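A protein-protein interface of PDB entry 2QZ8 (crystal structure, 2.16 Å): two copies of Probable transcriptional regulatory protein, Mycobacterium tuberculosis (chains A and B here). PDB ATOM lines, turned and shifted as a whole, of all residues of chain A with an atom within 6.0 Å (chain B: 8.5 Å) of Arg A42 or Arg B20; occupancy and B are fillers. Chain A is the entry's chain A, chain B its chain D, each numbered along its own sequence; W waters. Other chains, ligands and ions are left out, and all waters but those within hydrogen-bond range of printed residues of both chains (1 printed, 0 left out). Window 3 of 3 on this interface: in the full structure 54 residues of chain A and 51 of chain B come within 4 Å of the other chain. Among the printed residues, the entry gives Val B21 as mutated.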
ATOM      1  N   GLY A  19     -19.071  17.810 -17.390  1.00  0.00           N
ATOM      2  CA  GLY A  19     -20.124  17.339 -18.257  1.00  0.00           C
ATOM      3  C   GLY A  19     -19.911  17.729 -19.706  1.00  0.00           C
ATOM      4  O   GLY A  19     -20.518  17.135 -20.595  1.00  0.00           O
ATOM      5  N   ARG A  20     -19.054  18.714 -19.956  1.00  0.00           N
ATOM      6  CA  ARG A  20     -18.832  19.193 -21.324  1.00  0.00           C
ATOM      7  C   ARG A  20     -17.853  18.327 -22.122  1.00  0.00           C
ATOM      8  O   ARG A  20     -17.702  18.519 -23.339  1.00  0.00           O
ATOM      9  CB  ARG A  20     -18.343  20.643 -21.334  1.00  0.00           C
ATOM     10  CG  ARG A  20     -19.309  21.651 -20.726  1.00  0.00           C
ATOM     11  CD  ARG A  20     -18.608  22.979 -20.401  1.00  0.00           C
ATOM     12  NE  ARG A  20     -17.392  22.786 -19.610  1.00  0.00           N
ATOM     13  CZ  ARG A  20     -16.524  23.754 -19.325  1.00  0.00           C
ATOM     14  NH1 ARG A  20     -15.441  23.486 -18.605  1.00  0.00           N
ATOM     15  NH2 ARG A  20     -16.737  24.996 -19.760  1.00  0.00           N
ATOM     16  N   LEU A  23     -17.218  13.803 -27.146  1.00  0.00           N
ATOM     17  CA  LEU A  23     -17.122  12.401 -27.553  1.00  0.00           C
ATOM     18  C   LEU A  23     -15.689  11.987 -27.928  1.00  0.00           C
ATOM     19  O   LEU A  23     -15.249  10.867 -27.626  1.00  0.00           O
ATOM     20  CB  LEU A  23     -18.066  12.130 -28.725  1.00  0.00           C
ATOM     21  CG  LEU A  23     -19.549  12.427 -28.469  1.00  0.00           C
ATOM     22  CD1 LEU A  23     -20.357  12.266 -29.757  1.00  0.00           C
ATOM     23  CD2 LEU A  23     -20.099  11.517 -27.383  1.00  0.00           C
ATOM     24  N   VAL A  37     -18.440   5.319 -27.758  1.00  0.00           N
ATOM     25  CA  VAL A  37     -18.614   6.259 -26.656  1.00  0.00           C
ATOM     26  C   VAL A  37     -20.044   6.761 -26.655  1.00  0.00           C
ATOM     27  O   VAL A  37     -20.818   6.481 -25.743  1.00  0.00           O
ATOM     28  CB  VAL A  37     -17.668   7.470 -26.789  1.00  0.00           C
ATOM     29  CG1 VAL A  37     -18.133   8.611 -25.884  1.00  0.00           C
ATOM     30  CG2 VAL A  37     -16.230   7.056 -26.484  1.00  0.00           C
ATOM     31  N   GLN A  38     -20.388   7.494 -27.704  1.00  0.00           N
ATOM     32  CA  GLN A  38     -21.740   7.980 -27.916  1.00  0.00           C
ATOM     33  C   GLN A  38     -22.815   6.980 -27.472  1.00  0.00           C
ATOM     34  O   GLN A  38     -23.771   7.350 -26.790  1.00  0.00           O
ATOM     35  CB  GLN A  38     -21.915   8.328 -29.393  1.00  0.00           C
ATOM     36  CG  GLN A  38     -23.351   8.427 -29.862  1.00  0.00           C
ATOM     37  CD  GLN A  38     -23.933   9.807 -29.676  1.00  0.00           C
ATOM     38  OE1 GLN A  38     -24.358  10.171 -28.576  1.00  0.00           O
ATOM     39  NE2 GLN A  38     -23.971  10.587 -30.758  1.00  0.00           N
ATOM     40  N   SER A  39     -22.657   5.717 -27.857  1.00  0.00           N
ATOM     41  CA  SER A  39     -23.668   4.704 -27.555  1.00  0.00           C
ATOM     42  C   SER A  39     -23.711   4.365 -26.067  1.00  0.00           C
ATOM     43  O   SER A  39     -24.786   4.333 -25.462  1.00  0.00           O
ATOM     44  CB  SER A  39     -23.464   3.440 -28.408  1.00  0.00           C
ATOM     45  OG  SER A  39     -22.306   2.712 -28.022  1.00  0.00           O
ATOM     46  N   ARG A  40     -22.541   4.116 -25.485  1.00  0.00           N
ATOM     47  CA  ARG A  40     -22.436   3.874 -24.053  1.00  0.00           C
ATOM     48  C   ARG A  40     -23.016   5.049 -23.268  1.00  0.00           C
ATOM     49  O   ARG A  40     -23.814   4.857 -22.348  1.00  0.00           O
ATOM     50  CB  ARG A  40     -20.979   3.661 -23.646  1.00  0.00           C
ATOM     51  CG  ARG A  40     -20.408   2.299 -23.988  1.00  0.00           C
ATOM     52  CD  ARG A  40     -18.932   2.264 -23.626  1.00  0.00           C
ATOM     53  NE  ARG A  40     -18.311   0.957 -23.813  1.00  0.00           N
ATOM     54  CZ  ARG A  40     -18.361  -0.027 -22.921  1.00  0.00           C
ATOM     55  NH1 ARG A  40     -17.755  -1.183 -23.168  1.00  0.00           N
ATOM     56  NH2 ARG A  40     -19.020   0.141 -21.781  1.00  0.00           N
ATOM     57  N   VAL A  41     -22.610   6.263 -23.639  1.00  0.00           N
ATOM     58  CA  VAL A  41     -23.082   7.464 -22.965  1.00  0.00           C
ATOM     59  C   VAL A  41     -24.605   7.559 -23.030  1.00  0.00           C
ATOM     60  O   VAL A  41     -25.258   7.773 -22.009  1.00  0.00           O
ATOM     61  CB  VAL A  41     -22.439   8.749 -23.537  1.00  0.00           C
ATOM     62  CG1 VAL A  41     -23.034   9.976 -22.874  1.00  0.00           C
ATOM     63  CG2 VAL A  41     -20.949   8.727 -23.320  1.00  0.00           C
ATOM     64  N   ARG A  42     -25.182   7.390 -24.216  1.00  0.00           N
ATOM     65  CA  ARG A  42     -26.645   7.376 -24.314  1.00  0.00           C
ATOM     66  C   ARG A  42     -27.249   6.268 -23.437  1.00  0.00           C
ATOM     67  O   ARG A  42     -28.327   6.432 -22.860  1.00  0.00           O
ATOM     68  CB  ARG A  42     -27.117   7.273 -25.766  1.00  0.00           C
ATOM     69  CG  ARG A  42     -27.877   8.512 -26.261  1.00  0.00           C
ATOM     70  CD  ARG A  42     -27.369   9.819 -25.625  1.00  0.00           C
ATOM     71  NE  ARG A  42     -26.064  10.238 -26.143  1.00  0.00           N
ATOM     72  CZ  ARG A  42     -25.401  11.325 -25.746  1.00  0.00           C
ATOM     73  NH1 ARG A  42     -24.219  11.614 -26.282  1.00  0.00           N
ATOM     74  NH2 ARG A  42     -25.908  12.129 -24.818  1.00  0.00           N
ATOM     75  N   ARG A  43     -26.526   5.163 -23.311  1.00  0.00           N
ATOM     76  CA  ARG A  43     -26.962   4.057 -22.476  1.00  0.00           C
ATOM     77  C   ARG A  43     -26.964   4.477 -21.006  1.00  0.00           C
ATOM     78  O   ARG A  43     -27.982   4.366 -20.330  1.00  0.00           O
ATOM     79  CB  ARG A  43     -26.044   2.847 -22.680  1.00  0.00           C
ATOM     80  CG  ARG A  43     -26.696   1.499 -22.382  1.00  0.00           C
ATOM     81  CD  ARG A  43     -25.650   0.458 -22.006  1.00  0.00           C
ATOM     82  NE  ARG A  43     -25.304   0.558 -20.587  1.00  0.00           N
ATOM     83  CZ  ARG A  43     -24.272   1.246 -20.088  1.00  0.00           C
ATOM     84  NH1 ARG A  43     -23.432   1.916 -20.885  1.00  0.00           N
ATOM     85  NH2 ARG A  43     -24.080   1.255 -18.774  1.00  0.00           N
ATOM     86  N   LEU A  44     -25.814   4.954 -20.527  1.00  0.00           N
ATOM     87  CA  LEU A  44     -25.669   5.453 -19.165  1.00  0.00           C
ATOM     88  C   LEU A  44     -26.755   6.461 -18.826  1.00  0.00           C
ATOM     89  O   LEU A  44     -27.255   6.487 -17.705  1.00  0.00           O
ATOM     90  CB  LEU A  44     -24.289   6.092 -18.962  1.00  0.00           C
ATOM     91  CG  LEU A  44     -23.087   5.144 -18.871  1.00  0.00           C
ATOM     92  CD1 LEU A  44     -21.775   5.912 -18.786  1.00  0.00           C
ATOM     93  CD2 LEU A  44     -23.230   4.203 -17.696  1.00  0.00           C
ATOM     94  N   GLU A  45     -27.123   7.296 -19.791  1.00  0.00           N
ATOM     95  CA  GLU A  45     -28.176   8.277 -19.555  1.00  0.00           C
ATOM     96  C   GLU A  45     -29.542   7.585 -19.408  1.00  0.00           C
ATOM     97  O   GLU A  45     -30.339   7.919 -18.515  1.00  0.00           O
ATOM     98  CB  GLU A  45     -28.198   9.348 -20.666  1.00  0.00           C
ATOM     99  CG  GLU A  45     -26.970  10.278 -20.679  1.00  0.00           C
ATOM    100  CD  GLU A  45     -26.814  11.098 -21.971  1.00  0.00           C
ATOM    101  OE1 GLU A  45     -27.817  11.579 -22.523  1.00  0.00           O
ATOM    102  OE2 GLU A  45     -25.674  11.271 -22.432  1.00  0.00           O
ATOM    103  N   SER A  46     -29.811   6.609 -20.272  1.00  0.00           N
ATOM    104  CA  SER A  46     -31.119   5.959 -20.262  1.00  0.00           C
ATOM    105  C   SER A  46     -31.320   5.108 -19.004  1.00  0.00           C
ATOM    106  O   SER A  46     -32.411   5.079 -18.446  1.00  0.00           O
ATOM    107  CB  SER A  46     -31.327   5.123 -21.524  1.00  0.00           C
ATOM    108  OG  SER A  46     -30.430   4.031 -21.546  1.00  0.00           O
ATOM    109  N   ARG A  47     -30.262   4.431 -18.560  1.00  0.00           N
ATOM    110  CA  ARG A  47     -30.299   3.639 -17.328  1.00  0.00           C
ATOM    111  C   ARG A  47     -30.331   4.536 -16.095  1.00  0.00           C
ATOM    112  O   ARG A  47     -30.342   4.050 -14.964  1.00  0.00           O
ATOM    113  CB  ARG A  47     -29.081   2.721 -17.232  1.00  0.00           C
ATOM    114  CG  ARG A  47     -28.839   1.868 -18.449  1.00  0.00           C
ATOM    115  CD  ARG A  47     -27.439   1.279 -18.401  1.00  0.00           C
ATOM    116  NE  ARG A  47     -27.369   0.119 -17.518  1.00  0.00           N
ATOM    117  CZ  ARG A  47     -27.439  -1.141 -17.939  1.00  0.00           C
ATOM    118  NH1 ARG A  47     -27.373  -2.137 -17.062  1.00  0.00           N
ATOM    119  NH2 ARG A  47     -27.572  -1.408 -19.237  1.00  0.00           N
ATOM    120  N   TYR A  53     -27.001  17.263 -17.013  1.00  0.00           N
ATOM    121  CA  TYR A  53     -25.787  17.975 -17.398  1.00  0.00           C
ATOM    122  C   TYR A  53     -25.863  19.452 -17.040  1.00  0.00           C
ATOM    123  O   TYR A  53     -25.063  20.258 -17.532  1.00  0.00           O
ATOM    124  CB  TYR A  53     -25.577  17.860 -18.909  1.00  0.00           C
ATOM    125  CG  TYR A  53     -25.213  16.478 -19.382  1.00  0.00           C
ATOM    126  CD1 TYR A  53     -23.899  16.055 -19.373  1.00  0.00           C
ATOM    127  CD2 TYR A  53     -26.190  15.594 -19.842  1.00  0.00           C
ATOM    128  CE1 TYR A  53     -23.555  14.795 -19.809  1.00  0.00           C
ATOM    129  CE2 TYR A  53     -25.854  14.322 -20.284  1.00  0.00           C
ATOM    130  CZ  TYR A  53     -24.536  13.932 -20.265  1.00  0.00           C
ATOM    131  OH  TYR A  53     -24.158  12.683 -20.694  1.00  0.00           O
ATOM    132  N   GLU B  14     -29.449  29.279 -19.953  1.00  0.00           N
ATOM    133  CA  GLU B  14     -29.076  28.226 -20.885  1.00  0.00           C
ATOM    134  C   GLU B  14     -28.095  27.226 -20.284  1.00  0.00           C
ATOM    135  O   GLU B  14     -28.270  26.018 -20.437  1.00  0.00           O
ATOM    136  CB  GLU B  14     -28.503  28.830 -22.174  1.00  0.00           C
ATOM    137  CG  GLU B  14     -29.535  29.533 -23.035  1.00  0.00           C
ATOM    138  CD  GLU B  14     -30.462  28.548 -23.737  1.00  0.00           C
ATOM    139  OE1 GLU B  14     -29.969  27.488 -24.176  1.00  0.00           O
ATOM    140  OE2 GLU B  14     -31.679  28.828 -23.851  1.00  0.00           O
ATOM    141  N   LEU B  15     -27.059  27.723 -19.615  1.00  0.00           N
ATOM    142  CA  LEU B  15     -26.052  26.840 -19.031  1.00  0.00           C
ATOM    143  C   LEU B  15     -26.646  25.996 -17.911  1.00  0.00           C
ATOM    144  O   LEU B  15     -26.293  24.830 -17.748  1.00  0.00           O
ATOM    145  CB  LEU B  15     -24.882  27.649 -18.488  1.00  0.00           C
ATOM    146  CG  LEU B  15     -24.012  28.351 -19.533  1.00  0.00           C
ATOM    147  CD1 LEU B  15     -23.280  29.537 -18.913  1.00  0.00           C
ATOM    148  CD2 LEU B  15     -23.031  27.348 -20.131  1.00  0.00           C
ATOM    149  N   ALA B  16     -27.536  26.592 -17.123  1.00  0.00           N
ATOM    150  CA  ALA B  16     -28.192  25.849 -16.057  1.00  0.00           C
ATOM    151  C   ALA B  16     -29.143  24.810 -16.650  1.00  0.00           C
ATOM    152  O   ALA B  16     -29.384  23.780 -16.034  1.00  0.00           O
ATOM    153  CB  ALA B  16     -28.940  26.790 -15.114  1.00  0.00           C
ATOM    154  N   ALA B  17     -29.680  25.077 -17.842  1.00  0.00           N
ATOM    155  CA  ALA B  17     -30.578  24.122 -18.478  1.00  0.00           C
ATOM    156  C   ALA B  17     -29.784  22.959 -19.027  1.00  0.00           C
ATOM    157  O   ALA B  17     -30.254  21.824 -19.030  1.00  0.00           O
ATOM    158  CB  ALA B  17     -31.375  24.782 -19.582  1.00  0.00           C
ATOM    159  N   ASP B  18     -28.568  23.250 -19.489  1.00  0.00           N
ATOM    160  CA  ASP B  18     -27.687  22.237 -20.046  1.00  0.00           C
ATOM    161  C   ASP B  18     -26.263  22.795 -20.158  1.00  0.00           C
ATOM    162  O   ASP B  18     -26.002  23.698 -20.960  1.00  0.00           O
ATOM    163  CB  ASP B  18     -28.197  21.816 -21.427  1.00  0.00           C
ATOM    164  CG  ASP B  18     -27.468  20.613 -21.973  1.00  0.00           C
ATOM    165  OD1 ASP B  18     -27.950  20.035 -22.970  1.00  0.00           O
ATOM    166  OD2 ASP B  18     -26.414  20.237 -21.405  1.00  0.00           O
ATOM    167  N   GLY B  19     -25.347  22.244 -19.365  1.00  0.00           N
ATOM    168  CA  GLY B  19     -23.993  22.760 -19.277  1.00  0.00           C
ATOM    169  C   GLY B  19     -23.185  22.511 -20.532  1.00  0.00           C
ATOM    170  O   GLY B  19     -22.104  23.063 -20.688  1.00  0.00           O
ATOM    171  N   ARG B  20     -23.717  21.684 -21.429  1.00  0.00           N
ATOM    172  CA  ARG B  20     -23.032  21.336 -22.671  1.00  0.00           C
ATOM    173  C   ARG B  20     -23.351  22.308 -23.801  1.00  0.00           C
ATOM    174  O   ARG B  20     -22.752  22.251 -24.876  1.00  0.00           O
ATOM    175  CB  ARG B  20     -23.415  19.927 -23.107  1.00  0.00           C
ATOM    176  CG  ARG B  20     -23.092  18.832 -22.097  1.00  0.00           C
ATOM    177  CD  ARG B  20     -23.791  17.541 -22.486  1.00  0.00           C
ATOM    178  NE  ARG B  20     -25.243  17.725 -22.542  1.00  0.00           N
ATOM    179  CZ  ARG B  20     -26.103  16.801 -22.958  1.00  0.00           C
ATOM    180  NH1 ARG B  20     -27.403  17.071 -22.980  1.00  0.00           N
ATOM    181  NH2 ARG B  20     -25.661  15.613 -23.357  1.00  0.00           N
ATOM    182  N   VAL B  21     -24.309  23.195 -23.578  1.00  0.00           N
ATOM    183  CA  VAL B  21     -24.680  24.121 -24.642  1.00  0.00           C
ATOM    184  C   VAL B  21     -23.413  24.822 -25.169  1.00  0.00           C
ATOM    185  O   VAL B  21     -22.567  25.280 -24.395  1.00  0.00           O
ATOM    186  CB  VAL B  21     -25.734  25.126 -24.167  1.00  0.00           C
ATOM    187  CG1 VAL B  21     -25.215  25.899 -22.977  1.00  0.00           C
ATOM    188  CG2 VAL B  21     -26.145  26.050 -25.325  1.00  0.00           C
ATOM    189  N   THR B  22     -23.261  24.860 -26.488  1.00  0.00           N
ATOM    190  CA  THR B  22     -22.044  25.377 -27.096  1.00  0.00           C
ATOM    191  C   THR B  22     -22.026  26.899 -27.141  1.00  0.00           C
ATOM    192  O   THR B  22     -23.065  27.561 -27.008  1.00  0.00           O
ATOM    193  CB  THR B  22     -21.879  24.865 -28.537  1.00  0.00           C
ATOM    194  OG1 THR B  22     -22.894  25.466 -29.353  1.00  0.00           O
ATOM    195  CG2 THR B  22     -22.028  23.341 -28.590  1.00  0.00           C
ATOM    196  N   LEU B  23     -20.829  27.445 -27.326  1.00  0.00           N
ATOM    197  CA  LEU B  23     -20.644  28.875 -27.509  1.00  0.00           C
ATOM    198  C   LEU B  23     -21.476  29.381 -28.680  1.00  0.00           C
ATOM    199  O   LEU B  23     -22.047  30.470 -28.612  1.00  0.00           O
ATOM    200  CB  LEU B  23     -19.165  29.193 -27.750  1.00  0.00           C
ATOM    201  CG  LEU B  23     -18.275  28.849 -26.550  1.00  0.00           C
ATOM    202  CD1 LEU B  23     -16.830  28.782 -26.981  1.00  0.00           C
ATOM    203  CD2 LEU B  23     -18.473  29.872 -25.442  1.00  0.00           C
ATOM    204  N   SER B  24     -21.545  28.597 -29.750  1.00  0.00           N
ATOM    205  CA  SER B  24     -22.312  29.005 -30.927  1.00  0.00           C
ATOM    206  C   SER B  24     -23.804  29.014 -30.615  1.00  0.00           C
ATOM    207  O   SER B  24     -24.511  29.970 -30.934  1.00  0.00           O
ATOM    208  CB  SER B  24     -22.043  28.069 -32.101  1.00  0.00           C
ATOM    209  OG  SER B  24     -20.670  28.084 -32.435  1.00  0.00           O
ATOM    210  N   GLU B  25     -24.281  27.938 -30.001  1.00  0.00           N
ATOM    211  CA  GLU B  25     -25.649  27.904 -29.513  1.00  0.00           C
ATOM    212  C   GLU B  25     -25.949  29.096 -28.602  1.00  0.00           C
ATOM    213  O   GLU B  25     -26.951  29.781 -28.782  1.00  0.00           O
ATOM    214  CB  GLU B  25     -25.936  26.567 -28.822  1.00  0.00           C
ATOM    215  CG  GLU B  25     -26.030  25.432 -29.822  1.00  0.00           C
ATOM    216  CD  GLU B  25     -26.015  24.060 -29.194  1.00  0.00           C
ATOM    217  OE1 GLU B  25     -25.794  23.961 -27.968  1.00  0.00           O
ATOM    218  OE2 GLU B  25     -26.215  23.073 -29.939  1.00  0.00           O
ATOM    219  N   LEU B  26     -25.069  29.356 -27.639  1.00  0.00           N
ATOM    220  CA  LEU B  26     -25.261  30.483 -26.735  1.00  0.00           C
ATOM    221  C   LEU B  26     -25.279  31.813 -27.481  1.00  0.00           C
ATOM    222  O   LEU B  26     -26.145  32.665 -27.224  1.00  0.00           O
ATOM    223  CB  LEU B  26     -24.172  30.514 -25.666  1.00  0.00           C
ATOM    224  CG  LEU B  26     -24.234  29.387 -24.626  1.00  0.00           C
ATOM    225  CD1 LEU B  26     -23.015  29.404 -23.693  1.00  0.00           C
ATOM    226  CD2 LEU B  26     -25.542  29.469 -23.831  1.00  0.00           C
ATOM    227  N   ARG B  29     -28.493  32.314 -29.260  1.00  0.00           N
ATOM    228  CA  ARG B  29     -29.579  32.516 -28.320  1.00  0.00           C
ATOM    229  C   ARG B  29     -29.505  33.837 -27.577  1.00  0.00           C
ATOM    230  O   ARG B  29     -30.539  34.358 -27.151  1.00  0.00           O
ATOM    231  CB  ARG B  29     -29.667  31.352 -27.325  1.00  0.00           C
ATOM    232  CG  ARG B  29     -30.476  30.187 -27.863  1.00  0.00           C
ATOM    233  CD  ARG B  29     -29.682  28.922 -28.104  1.00  0.00           C
ATOM    234  NE  ARG B  29     -29.878  27.978 -27.017  1.00  0.00           N
ATOM    235  CZ  ARG B  29     -29.859  26.649 -27.139  1.00  0.00           C
ATOM    236  NH1 ARG B  29     -29.657  26.069 -28.311  1.00  0.00           N
ATOM    237  NH2 ARG B  29     -30.047  25.897 -26.066  1.00  0.00           N
ATOM    238  N   TYR B  53     -19.255  22.286 -14.088  1.00  0.00           N
ATOM    239  CA  TYR B  53     -20.002  21.668 -15.162  1.00  0.00           C
ATOM    240  C   TYR B  53     -20.092  20.156 -14.996  1.00  0.00           C
ATOM    241  O   TYR B  53     -20.406  19.436 -15.944  1.00  0.00           O
ATOM    242  CB  TYR B  53     -19.316  21.976 -16.484  1.00  0.00           C
ATOM    243  CG  TYR B  53     -19.356  23.424 -16.902  1.00  0.00           C
ATOM    244  CD1 TYR B  53     -20.393  23.905 -17.690  1.00  0.00           C
ATOM    245  CD2 TYR B  53     -18.339  24.300 -16.538  1.00  0.00           C
ATOM    246  CE1 TYR B  53     -20.428  25.226 -18.109  1.00  0.00           C
ATOM    247  CE2 TYR B  53     -18.357  25.634 -16.947  1.00  0.00           C
ATOM    248  CZ  TYR B  53     -19.405  26.082 -17.740  1.00  0.00           C
ATOM    249  OH  TYR B  53     -19.439  27.389 -18.154  1.00  0.00           O
ATOM    250  N   SER B  54     -19.807  19.667 -13.797  1.00  0.00           N
ATOM    251  CA  SER B  54     -19.848  18.226 -13.570  1.00  0.00           C
ATOM    252  C   SER B  54     -21.213  17.638 -13.950  1.00  0.00           C
ATOM    253  O   SER B  54     -22.249  18.197 -13.612  1.00  0.00           O
ATOM    254  CB  SER B  54     -19.514  17.919 -12.108  1.00  0.00           C
ATOM    255  OG  SER B  54     -20.284  18.737 -11.268  1.00  0.00           O
ATOM    256  N   ALA B  55     -21.215  16.522 -14.670  1.00  0.00           N
ATOM    257  CA  ALA B  55     -22.464  15.824 -14.945  1.00  0.00           C
ATOM    258  C   ALA B  55     -22.997  15.275 -13.623  1.00  0.00           C
ATOM    259  O   ALA B  55     -22.216  14.865 -12.784  1.00  0.00           O
ATOM    260  CB  ALA B  55     -22.238  14.697 -15.924  1.00  0.00           C
HETATM  261  O   HOH W   1     -19.146  26.665 -20.840  1.00  0.00           O
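Of the 15 printed residues of chain A, 4 touch a printed residue of chain B. Printed residues of chain A that touch a printed residue of chain B: Gly A19, Arg A20, Arg A42 and Tyr A53. Hydrophobic or aromatic side chains of chain A within 4 Å of the printed part of chain B: Tyr A53. Of the 17 printed residues of chain B, 6 touch a printed residue of chain A. Printed residues of chain B that touch a printed residue of chain A: Asp B18, Gly B19, Arg B20, Tyr B53, Ser B54 and Ala B55. Among the printed residues, 10 pairs touch across the chains. Among the printed residues, no Asp or Glu carboxylate lies within 4 Å of a Lys or Arg side-chain nitrogen of the other chain.
Gly A19 touches Arg B20, and with the chains exchanged Arg A20 touches Gly B19. Gly A19 touches Tyr B53, and with the chains exchanged Tyr A53 touches Gly B19. Arg A20 touches Tyr B53, and with the chains exchanged Tyr A53 touches Arg B20. Positions printed for both chains: 19, 20, 23 and 53.
Of chain B, only Arg B20 (3.8 Å) comes within 4 Å of Arg A42. Of chain A, only Gly A19, Arg A42 and Tyr A53 come within 4 Å of Arg B20. Of the printed residues of chain A, Ala B55 touches Gly A19. Of the printed residues of chain B, Arg A20 touches Gly B19 and Tyr B53. Of the printed residues of chain A, Asp B18 touches Tyr A53. Printed residues of chain B within 4 Å of Tyr A53: Asp B18 (3.5 Å), Gly B19 (2.7 Å) and Arg B20 (3.3 Å). Ala B17 touches none of the printed residues of chain A.
Water W1 bridges the side-chain hydroxyl (OH) of Tyr B53 (2.8 Å) and the guanidinium group (NH2) of Arg A20 (3.1 Å).
The side-chain carboxylate (OD2) of Asp B18 lies within salt-bridge range of the guanidinium group (NE) of Arg B20, 3.0 Å away. OE1 of Gln A38 sits at hydrogen-bond distance from NH1 of Arg A42 (2.7 Å). The guanidinium group (NH2) of Arg A42 is in salt-bridge range of the side-chain carboxylate (OE2) of Glu A45 (2.5 Å). The side-chain hydroxyl (OH) of Tyr A53 is in hydrogen-bond range of the side-chain carboxylate (OE2) of Glu A45, 2.7 Å away. The backbone carbonyl oxygen (O) of Arg A42 sits at hydrogen-bond distance from the side-chain hydroxyl (OG) of Ser A46, 3.5 Å away.
The backbone carbonyl oxygen of Tyr A53 sits at hydrogen-bond distance from the backbone NH of Gly B19, at 2.7 Å. N of Gly A19 sits at hydrogen-bond distance from O of Tyr B53, at 2.6 Å.
Among the printed residues, merely in contact across the chains: Arg A20 with Gly B19 (3.1 Å), Arg A20 with Tyr B53 (3.3 Å), Tyr A53 with Arg B20 (3.3 Å), Gly A19 with Arg B20 (3.4 Å), Tyr A53 with Asp B18 (3.5 Å), Gly A19 with Ala B55 (3.7 Å), Arg A42 with Arg B20 (3.8 Å) and Gly A19 with Ser B54 (3.9 Å).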
